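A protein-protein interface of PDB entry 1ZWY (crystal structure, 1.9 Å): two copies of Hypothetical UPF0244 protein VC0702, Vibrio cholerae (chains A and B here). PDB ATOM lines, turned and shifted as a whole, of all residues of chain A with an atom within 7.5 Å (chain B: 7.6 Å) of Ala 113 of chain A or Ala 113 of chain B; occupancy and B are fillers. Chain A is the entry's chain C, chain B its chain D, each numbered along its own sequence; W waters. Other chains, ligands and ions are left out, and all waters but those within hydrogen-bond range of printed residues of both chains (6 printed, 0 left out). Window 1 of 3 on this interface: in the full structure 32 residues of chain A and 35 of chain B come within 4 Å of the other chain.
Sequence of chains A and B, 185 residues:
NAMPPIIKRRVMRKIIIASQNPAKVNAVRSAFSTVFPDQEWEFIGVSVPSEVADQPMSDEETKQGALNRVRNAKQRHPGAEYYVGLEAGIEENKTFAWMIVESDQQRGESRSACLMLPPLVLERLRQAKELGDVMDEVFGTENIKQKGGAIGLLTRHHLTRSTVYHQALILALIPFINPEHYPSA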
ATOM      1  N   THR A  95       6.849 -17.363 -11.521  1.00  0.00           N
ATOM      2  CA  THR A  95       6.188 -16.092 -11.344  1.00  0.00           C
ATOM      3  C   THR A  95       7.208 -15.045 -10.895  1.00  0.00           C
ATOM      4  O   THR A  95       8.288 -15.384 -10.337  1.00  0.00           O
ATOM      5  CB  THR A  95       4.978 -16.179 -10.362  1.00  0.00           C
ATOM      6  OG1 THR A  95       4.213 -14.956 -10.418  1.00  0.00           O
ATOM      7  CG2 THR A  95       5.453 -16.423  -8.926  1.00  0.00           C
ATOM      8  N   PHE A  96       6.876 -13.782 -11.159  1.00  0.00           N
ATOM      9  CA  PHE A  96       7.800 -12.668 -10.953  1.00  0.00           C
ATOM     10  C   PHE A  96       6.974 -11.398 -11.111  1.00  0.00           C
ATOM     11  O   PHE A  96       5.794 -11.477 -11.450  1.00  0.00           O
ATOM     12  CB  PHE A  96       8.916 -12.685 -12.011  1.00  0.00           C
ATOM     13  CG  PHE A  96       8.389 -12.959 -13.406  1.00  0.00           C
ATOM     14  CD1 PHE A  96       7.738 -11.955 -14.116  1.00  0.00           C
ATOM     15  CD2 PHE A  96       8.444 -14.249 -13.947  1.00  0.00           C
ATOM     16  CE1 PHE A  96       7.175 -12.207 -15.369  1.00  0.00           C
ATOM     17  CE2 PHE A  96       7.888 -14.513 -15.201  1.00  0.00           C
ATOM     18  CZ  PHE A  96       7.262 -13.475 -15.917  1.00  0.00           C
ATOM     19  N   ALA A  97       7.590 -10.240 -10.882  1.00  0.00           N
ATOM     20  CA  ALA A  97       6.888  -8.964 -11.030  1.00  0.00           C
ATOM     21  C   ALA A  97       7.784  -7.983 -11.753  1.00  0.00           C
ATOM     22  O   ALA A  97       8.995  -7.966 -11.503  1.00  0.00           O
ATOM     23  CB  ALA A  97       6.502  -8.425  -9.694  1.00  0.00           C
ATOM     24  N   MET A  99       8.742  -4.157 -12.155  1.00  0.00           N
ATOM     25  CA  MET A  99       8.667  -2.801 -11.581  1.00  0.00           C
ATOM     26  C   MET A  99       9.092  -1.771 -12.630  1.00  0.00           C
ATOM     27  O   MET A  99      10.176  -1.901 -13.213  1.00  0.00           O
ATOM     28  CB  MET A  99       9.590  -2.690 -10.369  1.00  0.00           C
ATOM     29  CG  MET A  99       9.052  -3.382  -9.094  1.00  0.00           C
ATOM     30  SD  MET A  99       8.750  -5.323  -9.306  1.00  0.00           S
ATOM     31  CE  MET A  99       8.608  -5.783  -7.417  1.00  0.00           C
ATOM     32  N   SER A 110      13.053  -3.017 -13.391  1.00  0.00           N
ATOM     33  CA  SER A 110      13.681  -4.247 -12.937  1.00  0.00           C
ATOM     34  C   SER A 110      12.566  -5.279 -12.791  1.00  0.00           C
ATOM     35  O   SER A 110      11.461  -4.950 -12.394  1.00  0.00           O
ATOM     36  CB  SER A 110      14.371  -4.037 -11.574  1.00  0.00           C
ATOM     37  OG  SER A 110      15.010  -5.237 -11.076  1.00  0.00           O
ATOM     38  N   ARG A 111      12.908  -6.521 -13.093  1.00  0.00           N
ATOM     39  CA  ARG A 111      12.035  -7.653 -12.835  1.00  0.00           C
ATOM     40  C   ARG A 111      12.515  -8.354 -11.565  1.00  0.00           C
ATOM     41  O   ARG A 111      13.702  -8.658 -11.443  1.00  0.00           O
ATOM     42  CB  ARG A 111      12.111  -8.650 -13.984  1.00  0.00           C
ATOM     43  CG  ARG A 111      10.888  -9.558 -14.004  1.00  0.00           C
ATOM     44  CD  ARG A 111      10.974 -10.608 -15.078  1.00  0.00           C
ATOM     45  NE  ARG A 111      11.752 -11.774 -14.634  1.00  0.00           N
ATOM     46  CZ  ARG A 111      11.904 -12.880 -15.350  1.00  0.00           C
ATOM     47  NH1 ARG A 111      11.322 -12.981 -16.559  1.00  0.00           N
ATOM     48  NH2 ARG A 111      12.632 -13.880 -14.866  1.00  0.00           N
ATOM     49  N   SER A 112      11.593  -8.665 -10.664  1.00  0.00           N
ATOM     50  CA  SER A 112      11.966  -9.324  -9.409  1.00  0.00           C
ATOM     51  C   SER A 112      12.476 -10.740  -9.698  1.00  0.00           C
ATOM     52  O   SER A 112      12.193 -11.315 -10.761  1.00  0.00           O
ATOM     53  CB  SER A 112      10.786  -9.400  -8.394  1.00  0.00           C
ATOM     54  OG  SER A 112       9.690 -10.126  -8.936  1.00  0.00           O
ATOM     55  N   ALA A 113      13.208 -11.276  -8.740  1.00  0.00           N
ATOM     56  CA  ALA A 113      13.722 -12.628  -8.774  1.00  0.00           C
ATOM     57  C   ALA A 113      12.540 -13.588  -8.915  1.00  0.00           C
ATOM     58  O   ALA A 113      11.509 -13.443  -8.206  1.00  0.00           O
ATOM     59  CB  ALA A 113      14.504 -12.914  -7.484  1.00  0.00           C
ATOM     60  N   CYS A 114      12.647 -14.566  -9.822  1.00  0.00           N
ATOM     61  CA  CYS A 114      11.497 -15.440 -10.067  1.00  0.00           C
ATOM     62  C   CYS A 114      11.413 -16.653  -9.129  1.00  0.00           C
ATOM     63  O   CYS A 114      12.407 -17.095  -8.542  1.00  0.00           O
ATOM     64  CB  CYS A 114      11.368 -15.834 -11.552  1.00  0.00           C
ATOM     65  SG  CYS A 114      12.702 -16.910 -12.065  1.00  0.00           S
ATOM     66  N   LEU A 115      10.201 -17.153  -8.996  1.00  0.00           N
ATOM     67  CA  LEU A 115       9.766 -18.159  -7.990  1.00  0.00           C
ATOM     68  C   LEU A 115       9.166 -19.308  -8.824  1.00  0.00           C
ATOM     69  O   LEU A 115       8.306 -19.055  -9.640  1.00  0.00           O
ATOM     70  CB  LEU A 115       8.648 -17.518  -7.087  1.00  0.00           C
ATOM     71  CG  LEU A 115       7.753 -18.396  -6.188  1.00  0.00           C
ATOM     72  CD1 LEU A 115       8.435 -18.572  -4.869  1.00  0.00           C
ATOM     73  CD2 LEU A 115       6.352 -17.791  -5.901  1.00  0.00           C
ATOM     74  N   MET A 116       9.639 -20.531  -8.648  1.00  0.00           N
ATOM     75  CA  MET A 116       9.022 -21.707  -9.247  1.00  0.00           C
ATOM     76  C   MET A 116       7.749 -22.089  -8.490  1.00  0.00           C
ATOM     77  O   MET A 116       7.799 -22.279  -7.267  1.00  0.00           O
ATOM     78  CB  MET A 116       9.998 -22.881  -9.166  1.00  0.00           C
ATOM     79  CG  MET A 116      10.067 -23.742 -10.342  1.00  0.00           C
ATOM     80  SD  MET A 116      11.633 -24.965 -10.104  1.00  0.00           S
ATOM     81  CE  MET A 116      10.691 -26.315  -9.094  1.00  0.00           C
ATOM     82  N   ILE A 151       5.893 -16.249  -1.215  1.00  0.00           N
ATOM     83  CA  ILE A 151       7.344 -16.219  -0.992  1.00  0.00           C
ATOM     84  C   ILE A 151       7.660 -16.523   0.452  1.00  0.00           C
ATOM     85  O   ILE A 151       8.479 -17.390   0.742  1.00  0.00           O
ATOM     86  CB  ILE A 151       7.960 -14.866  -1.430  1.00  0.00           C
ATOM     87  CG1 ILE A 151       7.939 -14.765  -2.963  1.00  0.00           C
ATOM     88  CG2 ILE A 151       9.396 -14.719  -0.889  1.00  0.00           C
ATOM     89  CD1 ILE A 151       8.418 -13.404  -3.483  1.00  0.00           C
ATOM     90  N   LEU A 159      12.736 -15.349   3.179  1.00  0.00           N
ATOM     91  CA  LEU A 159      12.393 -14.180   2.343  1.00  0.00           C
ATOM     92  C   LEU A 159      10.922 -13.915   2.506  1.00  0.00           C
ATOM     93  O   LEU A 159      10.181 -14.801   2.973  1.00  0.00           O
ATOM     94  CB  LEU A 159      12.648 -14.485   0.866  1.00  0.00           C
ATOM     95  CG  LEU A 159      14.093 -14.828   0.470  1.00  0.00           C
ATOM     96  CD1 LEU A 159      14.108 -15.127  -1.020  1.00  0.00           C
ATOM     97  CD2 LEU A 159      15.050 -13.698   0.776  1.00  0.00           C
ATOM     98  N   VAL A 164      11.539  -9.199  -1.241  1.00  0.00           N
ATOM     99  CA  VAL A 164      11.890  -9.494  -2.667  1.00  0.00           C
ATOM    100  C   VAL A 164      11.532  -8.285  -3.552  1.00  0.00           C
ATOM    101  O   VAL A 164      12.330  -7.833  -4.421  1.00  0.00           O
ATOM    102  CB  VAL A 164      11.254 -10.831  -3.144  1.00  0.00           C
ATOM    103  CG1 VAL A 164      11.338 -10.999  -4.722  1.00  0.00           C
ATOM    104  CG2 VAL A 164      11.995 -12.018  -2.446  1.00  0.00           C
ATOM    105  N   TYR A 165      10.335  -7.746  -3.326  1.00  0.00           N
ATOM    106  CA  TYR A 165       9.906  -6.552  -4.028  1.00  0.00           C
ATOM    107  C   TYR A 165      10.815  -5.369  -3.830  1.00  0.00           C
ATOM    108  O   TYR A 165      11.060  -4.610  -4.806  1.00  0.00           O
ATOM    109  CB  TYR A 165       8.461  -6.199  -3.668  1.00  0.00           C
ATOM    110  CG  TYR A 165       7.438  -7.038  -4.441  1.00  0.00           C
ATOM    111  CD1 TYR A 165       7.807  -8.218  -5.100  1.00  0.00           C
ATOM    112  CD2 TYR A 165       6.104  -6.647  -4.505  1.00  0.00           C
ATOM    113  CE1 TYR A 165       6.890  -8.969  -5.805  1.00  0.00           C
ATOM    114  CE2 TYR A 165       5.176  -7.411  -5.196  1.00  0.00           C
ATOM    115  CZ  TYR A 165       5.588  -8.555  -5.863  1.00  0.00           C
ATOM    116  OH  TYR A 165       4.651  -9.308  -6.558  1.00  0.00           O
ATOM    117  N   GLN A 167      13.984  -5.223  -3.300  1.00  0.00           N
ATOM    118  CA  GLN A 167      15.189  -5.267  -4.126  1.00  0.00           C
ATOM    119  C   GLN A 167      14.924  -4.774  -5.558  1.00  0.00           C
ATOM    120  O   GLN A 167      15.704  -3.990  -6.101  1.00  0.00           O
ATOM    121  CB  GLN A 167      15.819  -6.689  -4.130  1.00  0.00           C
ATOM    122  CG  GLN A 167      16.458  -7.024  -2.795  1.00  0.00           C
ATOM    123  CD  GLN A 167      17.604  -8.024  -2.868  1.00  0.00           C
ATOM    124  OE1 GLN A 167      17.868  -8.611  -3.920  1.00  0.00           O
ATOM    125  NE2 GLN A 167      18.308  -8.199  -1.733  1.00  0.00           N
ATOM    126  N   ALA A 168      13.857  -5.258  -6.181  1.00  0.00           N
ATOM    127  CA  ALA A 168      13.585  -4.879  -7.589  1.00  0.00           C
ATOM    128  C   ALA A 168      13.216  -3.390  -7.677  1.00  0.00           C
ATOM    129  O   ALA A 168      13.613  -2.696  -8.620  1.00  0.00           O
ATOM    130  CB  ALA A 168      12.464  -5.758  -8.154  1.00  0.00           C
ATOM    131  N   LEU A 169      12.488  -2.887  -6.676  1.00  0.00           N
ATOM    132  CA  LEU A 169      12.166  -1.435  -6.625  1.00  0.00           C
ATOM    133  C   LEU A 169      13.412  -0.563  -6.498  1.00  0.00           C
ATOM    134  O   LEU A 169      13.553   0.437  -7.204  1.00  0.00           O
ATOM    135  CB  LEU A 169      11.167  -1.147  -5.501  1.00  0.00           C
ATOM    136  CG  LEU A 169       9.734  -1.534  -5.859  1.00  0.00           C
ATOM    137  CD1 LEU A 169       8.892  -1.582  -4.558  1.00  0.00           C
ATOM    138  CD2 LEU A 169       9.191  -0.470  -6.846  1.00  0.00           C
ATOM    139  N   LEU A 171      16.459  -1.486  -7.501  1.00  0.00           N
ATOM    140  CA  LEU A 171      17.140  -1.606  -8.815  1.00  0.00           C
ATOM    141  C   LEU A 171      16.447  -0.710  -9.841  1.00  0.00           C
ATOM    142  O   LEU A 171      17.100  -0.116 -10.677  1.00  0.00           O
ATOM    143  CB  LEU A 171      17.159  -3.066  -9.297  1.00  0.00           C
ATOM    144  CG  LEU A 171      18.097  -3.999  -8.509  1.00  0.00           C
ATOM    145  CD1 LEU A 171      17.821  -5.507  -8.845  1.00  0.00           C
ATOM    146  CD2 LEU A 171      19.585  -3.658  -8.693  1.00  0.00           C
ATOM    147  N   THR B  95      21.075  -7.183 -17.115  1.00  0.00           N
ATOM    148  CA  THR B  95      21.921  -8.287 -16.667  1.00  0.00           C
ATOM    149  C   THR B  95      21.306  -8.953 -15.409  1.00  0.00           C
ATOM    150  O   THR B  95      20.544  -8.316 -14.691  1.00  0.00           O
ATOM    151  CB  THR B  95      23.390  -7.811 -16.450  1.00  0.00           C
ATOM    152  OG1 THR B  95      24.228  -8.962 -16.339  1.00  0.00           O
ATOM    153  CG2 THR B  95      23.485  -7.023 -15.167  1.00  0.00           C
ATOM    154  N   PHE B  96      21.632 -10.219 -15.164  1.00  0.00           N
ATOM    155  CA  PHE B  96      20.935 -11.051 -14.153  1.00  0.00           C
ATOM    156  C   PHE B  96      21.790 -12.299 -14.074  1.00  0.00           C
ATOM    157  O   PHE B  96      22.772 -12.405 -14.815  1.00  0.00           O
ATOM    158  CB  PHE B  96      19.502 -11.410 -14.638  1.00  0.00           C
ATOM    159  CG  PHE B  96      19.455 -11.813 -16.100  1.00  0.00           C
ATOM    160  CD1 PHE B  96      19.897 -13.089 -16.490  1.00  0.00           C
ATOM    161  CD2 PHE B  96      19.042 -10.889 -17.089  1.00  0.00           C
ATOM    162  CE1 PHE B  96      19.904 -13.456 -17.818  1.00  0.00           C
ATOM    163  CE2 PHE B  96      19.049 -11.243 -18.435  1.00  0.00           C
ATOM    164  CZ  PHE B  96      19.469 -12.538 -18.801  1.00  0.00           C
ATOM    165  N   ALA B  97      21.415 -13.241 -13.218  1.00  0.00           N
ATOM    166  CA  ALA B  97      22.065 -14.529 -13.147  1.00  0.00           C
ATOM    167  C   ALA B  97      21.020 -15.606 -12.905  1.00  0.00           C
ATOM    168  O   ALA B  97      20.049 -15.363 -12.187  1.00  0.00           O
ATOM    169  CB  ALA B  97      23.128 -14.541 -12.003  1.00  0.00           C
ATOM    170  N   MET B  99      20.333 -19.132 -11.184  1.00  0.00           N
ATOM    171  CA  MET B  99      20.699 -20.090 -10.159  1.00  0.00           C
ATOM    172  C   MET B  99      20.001 -21.430 -10.436  1.00  0.00           C
ATOM    173  O   MET B  99      18.768 -21.500 -10.566  1.00  0.00           O
ATOM    174  CB  MET B  99      20.280 -19.612  -8.757  1.00  0.00           C
ATOM    175  CG  MET B  99      21.017 -18.437  -8.160  1.00  0.00           C
ATOM    176  SD  MET B  99      21.315 -16.899  -9.380  1.00  0.00           S
ATOM    177  CE  MET B  99      22.306 -15.704  -8.151  1.00  0.00           C
ATOM    178  N   SER B 110      16.017 -20.254 -10.041  1.00  0.00           N
ATOM    179  CA  SER B 110      15.594 -18.881  -9.908  1.00  0.00           C
ATOM    180  C   SER B 110      16.563 -18.007 -10.725  1.00  0.00           C
ATOM    181  O   SER B 110      17.777 -18.242 -10.720  1.00  0.00           O
ATOM    182  CB  SER B 110      15.639 -18.439  -8.439  1.00  0.00           C
ATOM    183  OG  SER B 110      15.220 -17.060  -8.262  1.00  0.00           O
ATOM    184  N   ARG B 111      15.998 -17.005 -11.399  1.00  0.00           N
ATOM    185  CA  ARG B 111      16.780 -15.946 -12.001  1.00  0.00           C
ATOM    186  C   ARG B 111      16.762 -14.733 -11.089  1.00  0.00           C
ATOM    187  O   ARG B 111      15.666 -14.249 -10.680  1.00  0.00           O
ATOM    188  CB  ARG B 111      16.181 -15.555 -13.356  1.00  0.00           C
ATOM    189  CG  ARG B 111      17.196 -14.814 -14.260  1.00  0.00           C
ATOM    190  CD  ARG B 111      16.562 -14.292 -15.543  1.00  0.00           C
ATOM    191  NE  ARG B 111      15.936 -12.970 -15.391  1.00  0.00           N
ATOM    192  CZ  ARG B 111      15.349 -12.309 -16.390  1.00  0.00           C
ATOM    193  NH1 ARG B 111      15.310 -12.864 -17.614  1.00  0.00           N
ATOM    194  NH2 ARG B 111      14.771 -11.106 -16.174  1.00  0.00           N
ATOM    195  N   SER B 112      17.940 -14.153 -10.841  1.00  0.00           N
ATOM    196  CA  SER B 112      18.027 -12.998  -9.964  1.00  0.00           C
ATOM    197  C   SER B 112      17.345 -11.768 -10.538  1.00  0.00           C
ATOM    198  O   SER B 112      17.115 -11.673 -11.753  1.00  0.00           O
ATOM    199  CB  SER B 112      19.492 -12.632  -9.645  1.00  0.00           C
ATOM    200  OG  SER B 112      20.182 -12.310 -10.854  1.00  0.00           O
ATOM    201  N   ALA B 113      17.044 -10.820  -9.658  1.00  0.00           N
ATOM    202  CA  ALA B 113      16.474  -9.540 -10.080  1.00  0.00           C
ATOM    203  C   ALA B 113      17.410  -8.858 -11.080  1.00  0.00           C
ATOM    204  O   ALA B 113      18.648  -8.880 -10.897  1.00  0.00           O
ATOM    205  CB  ALA B 113      16.260  -8.659  -8.890  1.00  0.00           C
ATOM    206  N   CYS B 114      16.861  -8.271 -12.144  1.00  0.00           N
ATOM    207  CA  CYS B 114      17.746  -7.758 -13.228  1.00  0.00           C
ATOM    208  C   CYS B 114      18.090  -6.275 -13.059  1.00  0.00           C
ATOM    209  O   CYS B 114      17.313  -5.474 -12.516  1.00  0.00           O
ATOM    210  CB  CYS B 114      17.184  -8.053 -14.637  1.00  0.00           C
ATOM    211  SG  CYS B 114      15.564  -7.253 -14.949  1.00  0.00           S
ATOM    212  N   LEU B 115      19.291  -5.930 -13.495  1.00  0.00           N
ATOM    213  CA  LEU B 115      19.824  -4.588 -13.448  1.00  0.00           C
ATOM    214  C   LEU B 115      19.753  -3.991 -14.860  1.00  0.00           C
ATOM    215  O   LEU B 115      20.206  -4.608 -15.802  1.00  0.00           O
ATOM    216  CB  LEU B 115      21.313  -4.673 -13.054  1.00  0.00           C
ATOM    217  CG  LEU B 115      22.129  -3.408 -13.377  1.00  0.00           C
ATOM    218  CD1 LEU B 115      21.714  -2.243 -12.501  1.00  0.00           C
ATOM    219  CD2 LEU B 115      23.612  -3.683 -13.233  1.00  0.00           C
ATOM    220  N   MET B 116      19.213  -2.788 -14.987  1.00  0.00           N
ATOM    221  CA  MET B 116      19.224  -2.089 -16.268  1.00  0.00           C
ATOM    222  C   MET B 116      20.561  -1.378 -16.492  1.00  0.00           C
ATOM    223  O   MET B 116      21.000  -0.563 -15.672  1.00  0.00           O
ATOM    224  CB  MET B 116      18.065  -1.099 -16.326  1.00  0.00           C
ATOM    225  CG  MET B 116      17.723  -0.701 -17.759  1.00  0.00           C
ATOM    226  SD  MET B 116      16.372   0.751 -17.769  1.00  0.00           S
ATOM    227  CE  MET B 116      17.422   2.164 -17.079  1.00  0.00           C
ATOM    228  N   ILE B 151      26.639  -2.940  -8.740  1.00  0.00           N
ATOM    229  CA  ILE B 151      25.347  -2.819  -8.034  1.00  0.00           C
ATOM    230  C   ILE B 151      25.492  -1.977  -6.775  1.00  0.00           C
ATOM    231  O   ILE B 151      24.705  -1.066  -6.552  1.00  0.00           O
ATOM    232  CB  ILE B 151      24.638  -4.165  -7.759  1.00  0.00           C
ATOM    233  CG1 ILE B 151      24.005  -4.682  -9.046  1.00  0.00           C
ATOM    234  CG2 ILE B 151      23.506  -3.985  -6.684  1.00  0.00           C
ATOM    235  CD1 ILE B 151      23.704  -6.213  -9.006  1.00  0.00           C
ATOM    236  N   LEU B 159      22.015  -2.225  -2.209  1.00  0.00           N
ATOM    237  CA  LEU B 159      22.170  -3.592  -2.637  1.00  0.00           C
ATOM    238  C   LEU B 159      23.591  -3.812  -3.067  1.00  0.00           C
ATOM    239  O   LEU B 159      24.324  -2.861  -3.371  1.00  0.00           O
ATOM    240  CB  LEU B 159      21.265  -3.934  -3.835  1.00  0.00           C
ATOM    241  CG  LEU B 159      19.770  -3.714  -3.631  1.00  0.00           C
ATOM    242  CD1 LEU B 159      19.059  -3.761  -4.987  1.00  0.00           C
ATOM    243  CD2 LEU B 159      19.211  -4.792  -2.651  1.00  0.00           C
ATOM    244  N   VAL B 164      21.778  -9.566  -3.809  1.00  0.00           N
ATOM    245  CA  VAL B 164      20.845  -9.892  -4.893  1.00  0.00           C
ATOM    246  C   VAL B 164      20.934 -11.410  -5.214  1.00  0.00           C
ATOM    247  O   VAL B 164      19.905 -12.073  -5.346  1.00  0.00           O
ATOM    248  CB  VAL B 164      21.100  -8.972  -6.149  1.00  0.00           C
ATOM    249  CG1 VAL B 164      20.338  -9.503  -7.376  1.00  0.00           C
ATOM    250  CG2 VAL B 164      20.698  -7.499  -5.813  1.00  0.00           C
ATOM    251  N   TYR B 165      22.142 -11.962  -5.326  1.00  0.00           N
ATOM    252  CA  TYR B 165      22.324 -13.395  -5.588  1.00  0.00           C
ATOM    253  C   TYR B 165      21.759 -14.233  -4.438  1.00  0.00           C
ATOM    254  O   TYR B 165      21.214 -15.292  -4.676  1.00  0.00           O
ATOM    255  CB  TYR B 165      23.822 -13.762  -5.802  1.00  0.00           C
ATOM    256  CG  TYR B 165      24.397 -13.425  -7.213  1.00  0.00           C
ATOM    257  CD1 TYR B 165      23.707 -12.603  -8.100  1.00  0.00           C
ATOM    258  CD2 TYR B 165      25.644 -13.930  -7.614  1.00  0.00           C
ATOM    259  CE1 TYR B 165      24.222 -12.304  -9.384  1.00  0.00           C
ATOM    260  CE2 TYR B 165      26.175 -13.639  -8.891  1.00  0.00           C
ATOM    261  CZ  TYR B 165      25.460 -12.841  -9.771  1.00  0.00           C
ATOM    262  OH  TYR B 165      25.999 -12.535 -11.032  1.00  0.00           O
ATOM    263  N   GLN B 167      19.115 -13.793  -2.547  1.00  0.00           N
ATOM    264  CA  GLN B 167      17.670 -14.007  -2.629  1.00  0.00           C
ATOM    265  C   GLN B 167      17.347 -15.034  -3.722  1.00  0.00           C
ATOM    266  O   GLN B 167      16.489 -15.887  -3.538  1.00  0.00           O
ATOM    267  CB  GLN B 167      16.962 -12.694  -2.915  1.00  0.00           C
ATOM    268  CG  GLN B 167      17.083 -11.659  -1.780  1.00  0.00           C
ATOM    269  CD  GLN B 167      15.890 -10.705  -1.813  1.00  0.00           C
ATOM    270  OE1 GLN B 167      15.270 -10.532  -2.866  1.00  0.00           O
ATOM    271  NE2 GLN B 167      15.612 -10.035  -0.673  1.00  0.00           N
ATOM    272  N   ALA B 168      18.070 -14.982  -4.846  1.00  0.00           N
ATOM    273  CA  ALA B 168      17.829 -15.938  -5.944  1.00  0.00           C
ATOM    274  C   ALA B 168      18.219 -17.383  -5.551  1.00  0.00           C
ATOM    275  O   ALA B 168      17.498 -18.336  -5.856  1.00  0.00           O
ATOM    276  CB  ALA B 168      18.574 -15.497  -7.228  1.00  0.00           C
ATOM    277  N   LEU B 169      19.316 -17.535  -4.825  1.00  0.00           N
ATOM    278  CA  LEU B 169      19.692 -18.869  -4.282  1.00  0.00           C
ATOM    279  C   LEU B 169      18.627 -19.447  -3.322  1.00  0.00           C
ATOM    280  O   LEU B 169      18.262 -20.611  -3.419  1.00  0.00           O
ATOM    281  CB  LEU B 169      21.076 -18.777  -3.618  1.00  0.00           C
ATOM    282  CG  LEU B 169      22.232 -18.772  -4.637  1.00  0.00           C
ATOM    283  CD1 LEU B 169      23.544 -18.271  -3.956  1.00  0.00           C
ATOM    284  CD2 LEU B 169      22.475 -20.147  -5.259  1.00  0.00           C
ATOM    285  N   LEU B 171      15.424 -18.648  -3.284  1.00  0.00           N
ATOM    286  CA  LEU B 171      14.280 -19.037  -4.147  1.00  0.00           C
ATOM    287  C   LEU B 171      14.526 -20.362  -4.907  1.00  0.00           C
ATOM    288  O   LEU B 171      13.603 -21.174  -5.086  1.00  0.00           O
ATOM    289  CB  LEU B 171      13.886 -17.902  -5.105  1.00  0.00           C
ATOM    290  CG  LEU B 171      13.397 -16.629  -4.382  1.00  0.00           C
ATOM    291  CD1 LEU B 171      13.321 -15.506  -5.397  1.00  0.00           C
ATOM    292  CD2 LEU B 171      11.989 -16.818  -3.695  1.00  0.00           C
HETATM  293  O   HOH W   1      13.444 -12.947 -12.395  1.00  0.00           O
HETATM  294  O   HOH W   2      15.107 -10.801 -13.443  1.00  0.00           O
HETATM  295  O   HOH W   3      17.539  -1.649 -12.999  1.00  0.00           O
HETATM  296  O   HOH W   4      15.985 -10.116  -5.352  1.00  0.00           O
HETATM  297  O   HOH W   5      13.433 -15.770 -17.432  1.00  0.00           O
HETATM  298  O   HOH W   6      12.162 -21.032  -7.304  1.00  0.00           O
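The backbone carbonyl oxygen of Cys 114 of chain B is in hydrogen-bond range of the side-chain hydroxyl of Ser 110 of chain A (2.7 Å).
The backbone NH (N) of Cys 114 of chain B is in hydrogen-bond range of the backbone carbonyl oxygen (O) of Arg 111 of chain A (3.3 Å).
The backbone carbonyl oxygen of Cys 114 of chain A sits at hydrogen-bond distance from the side-chain hydroxyl of Ser 110 of chain B, at 2.8 Å.
The backbone carbonyl oxygen (O) of Arg 111 of chain B is in hydrogen-bond range of the backbone NH (N) of Cys 114 of chain A, 3.2 Å away.
The side-chain amide oxygen (OE1) of Gln 167 of chain A lies close to the side-chain amide oxygen (OE1) of Gln 167 of chain B (3.4 Å).
NE of Arg 111 of chain A sits close to NH2 of Arg 111 of chain B (3.5 Å).
N of Met 99 of chain A sits at hydrogen-bond distance from O of Ser 110 of chain A (2.8 Å).
N of Met 99 of chain B is in hydrogen-bond range of O of Ser 110 of chain B (2.7 Å).
Arg 111 of chain A touches Ala 113 of chain B.
Ala 113 of chain B touches Ala 113 of chain A (N to CA, 3.9 Å).
Leu 171 of chain B touches Ala 113 of chain A (CD1 to CB, 3.5 Å).
Gln 167 of chain B touches Leu 159 of chain A (O to CD1, 3.5 Å).
Leu 159 of chain B touches Gln 167 of chain A (CD1 to O, 3.5 Å).
Gln 167 of chain A touches Val 164 of chain B.
Leu 171 of chain A touches Leu 159 of chain B.
Ala 113 of chain B touches just these residues of chain A: Arg 111, Ala 113 and Leu 171.
Of the printed residues of chain A, Leu 159 of chain B touches Gln 167 (3.5 Å) and Leu 171 (3.7 Å).
Printed residues of chain A within 4 Å of Ser 110 of chain B: Cys 114 (2.8 Å).
Printed residues of chain B within 4 Å of Leu 159 of chain A: Gln 167 (3.5 Å) and Leu 171 (3.8 Å).
Ala 97 of chain B touches none of the printed residues of chain A.
The nearest residue of chain B that does not touch Ala 113 of chain A is Ser 112 of chain B (4.1 Å).
The nearest printed residue of chain B that does not touch Gln 167 of chain A is Ala 113 of chain B (5.2 Å).
Hydrophobic or aromatic side chains of chain A that line the printed part of chain B: Ala 113, Leu 159, Val 164 and Leu 171.
Along chain A the printed residues that touch a printed residue of chain B span positions 110 to 171.
Of the 19 printed residues of chain B, 8 touch a printed residue of chain A.
Hydrophobic or aromatic side chains of chain B that line the printed part of chain A: Ala 113, Leu 159, Val 164 and Leu 171.
Along chain B the printed residues that touch a printed residue of chain A span positions 110 to 171.
Among the printed residues, no Asp or Glu carboxylate lies within 4 Å of a Lys or Arg side-chain nitrogen of the other chain.
Ser 110 of chain A touches Cys 114 of chain B, and with the chains exchanged Cys 114 of chain A touches Ser 110 of chain B.
Arg 111 of chain A touches Cys 114 of chain B, and with the chains exchanged Cys 114 of chain A touches Arg 111 of chain B.
Positions printed for both chains: 95, 96, 97, 99, 110, 111, 112, 113, 114, 115, 116, 151, 159, 164, 165, 167, 168, 169 and 171.
Water W1 lies within hydrogen-bond range of the backbone carbonyl oxygen (O) of Ser 112 of chain A, the guanidinium group (NH2) of Arg 111 of chain A, the backbone carbonyl oxygen (O) of Arg 111 of chain B and the backbone NH (N) of Cys 114 of chain A.
Water W5 bridges the guanidinium group (NH2) of Arg 111 of chain A and the guanidinium group (NH1) of Arg 111 of chain B.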
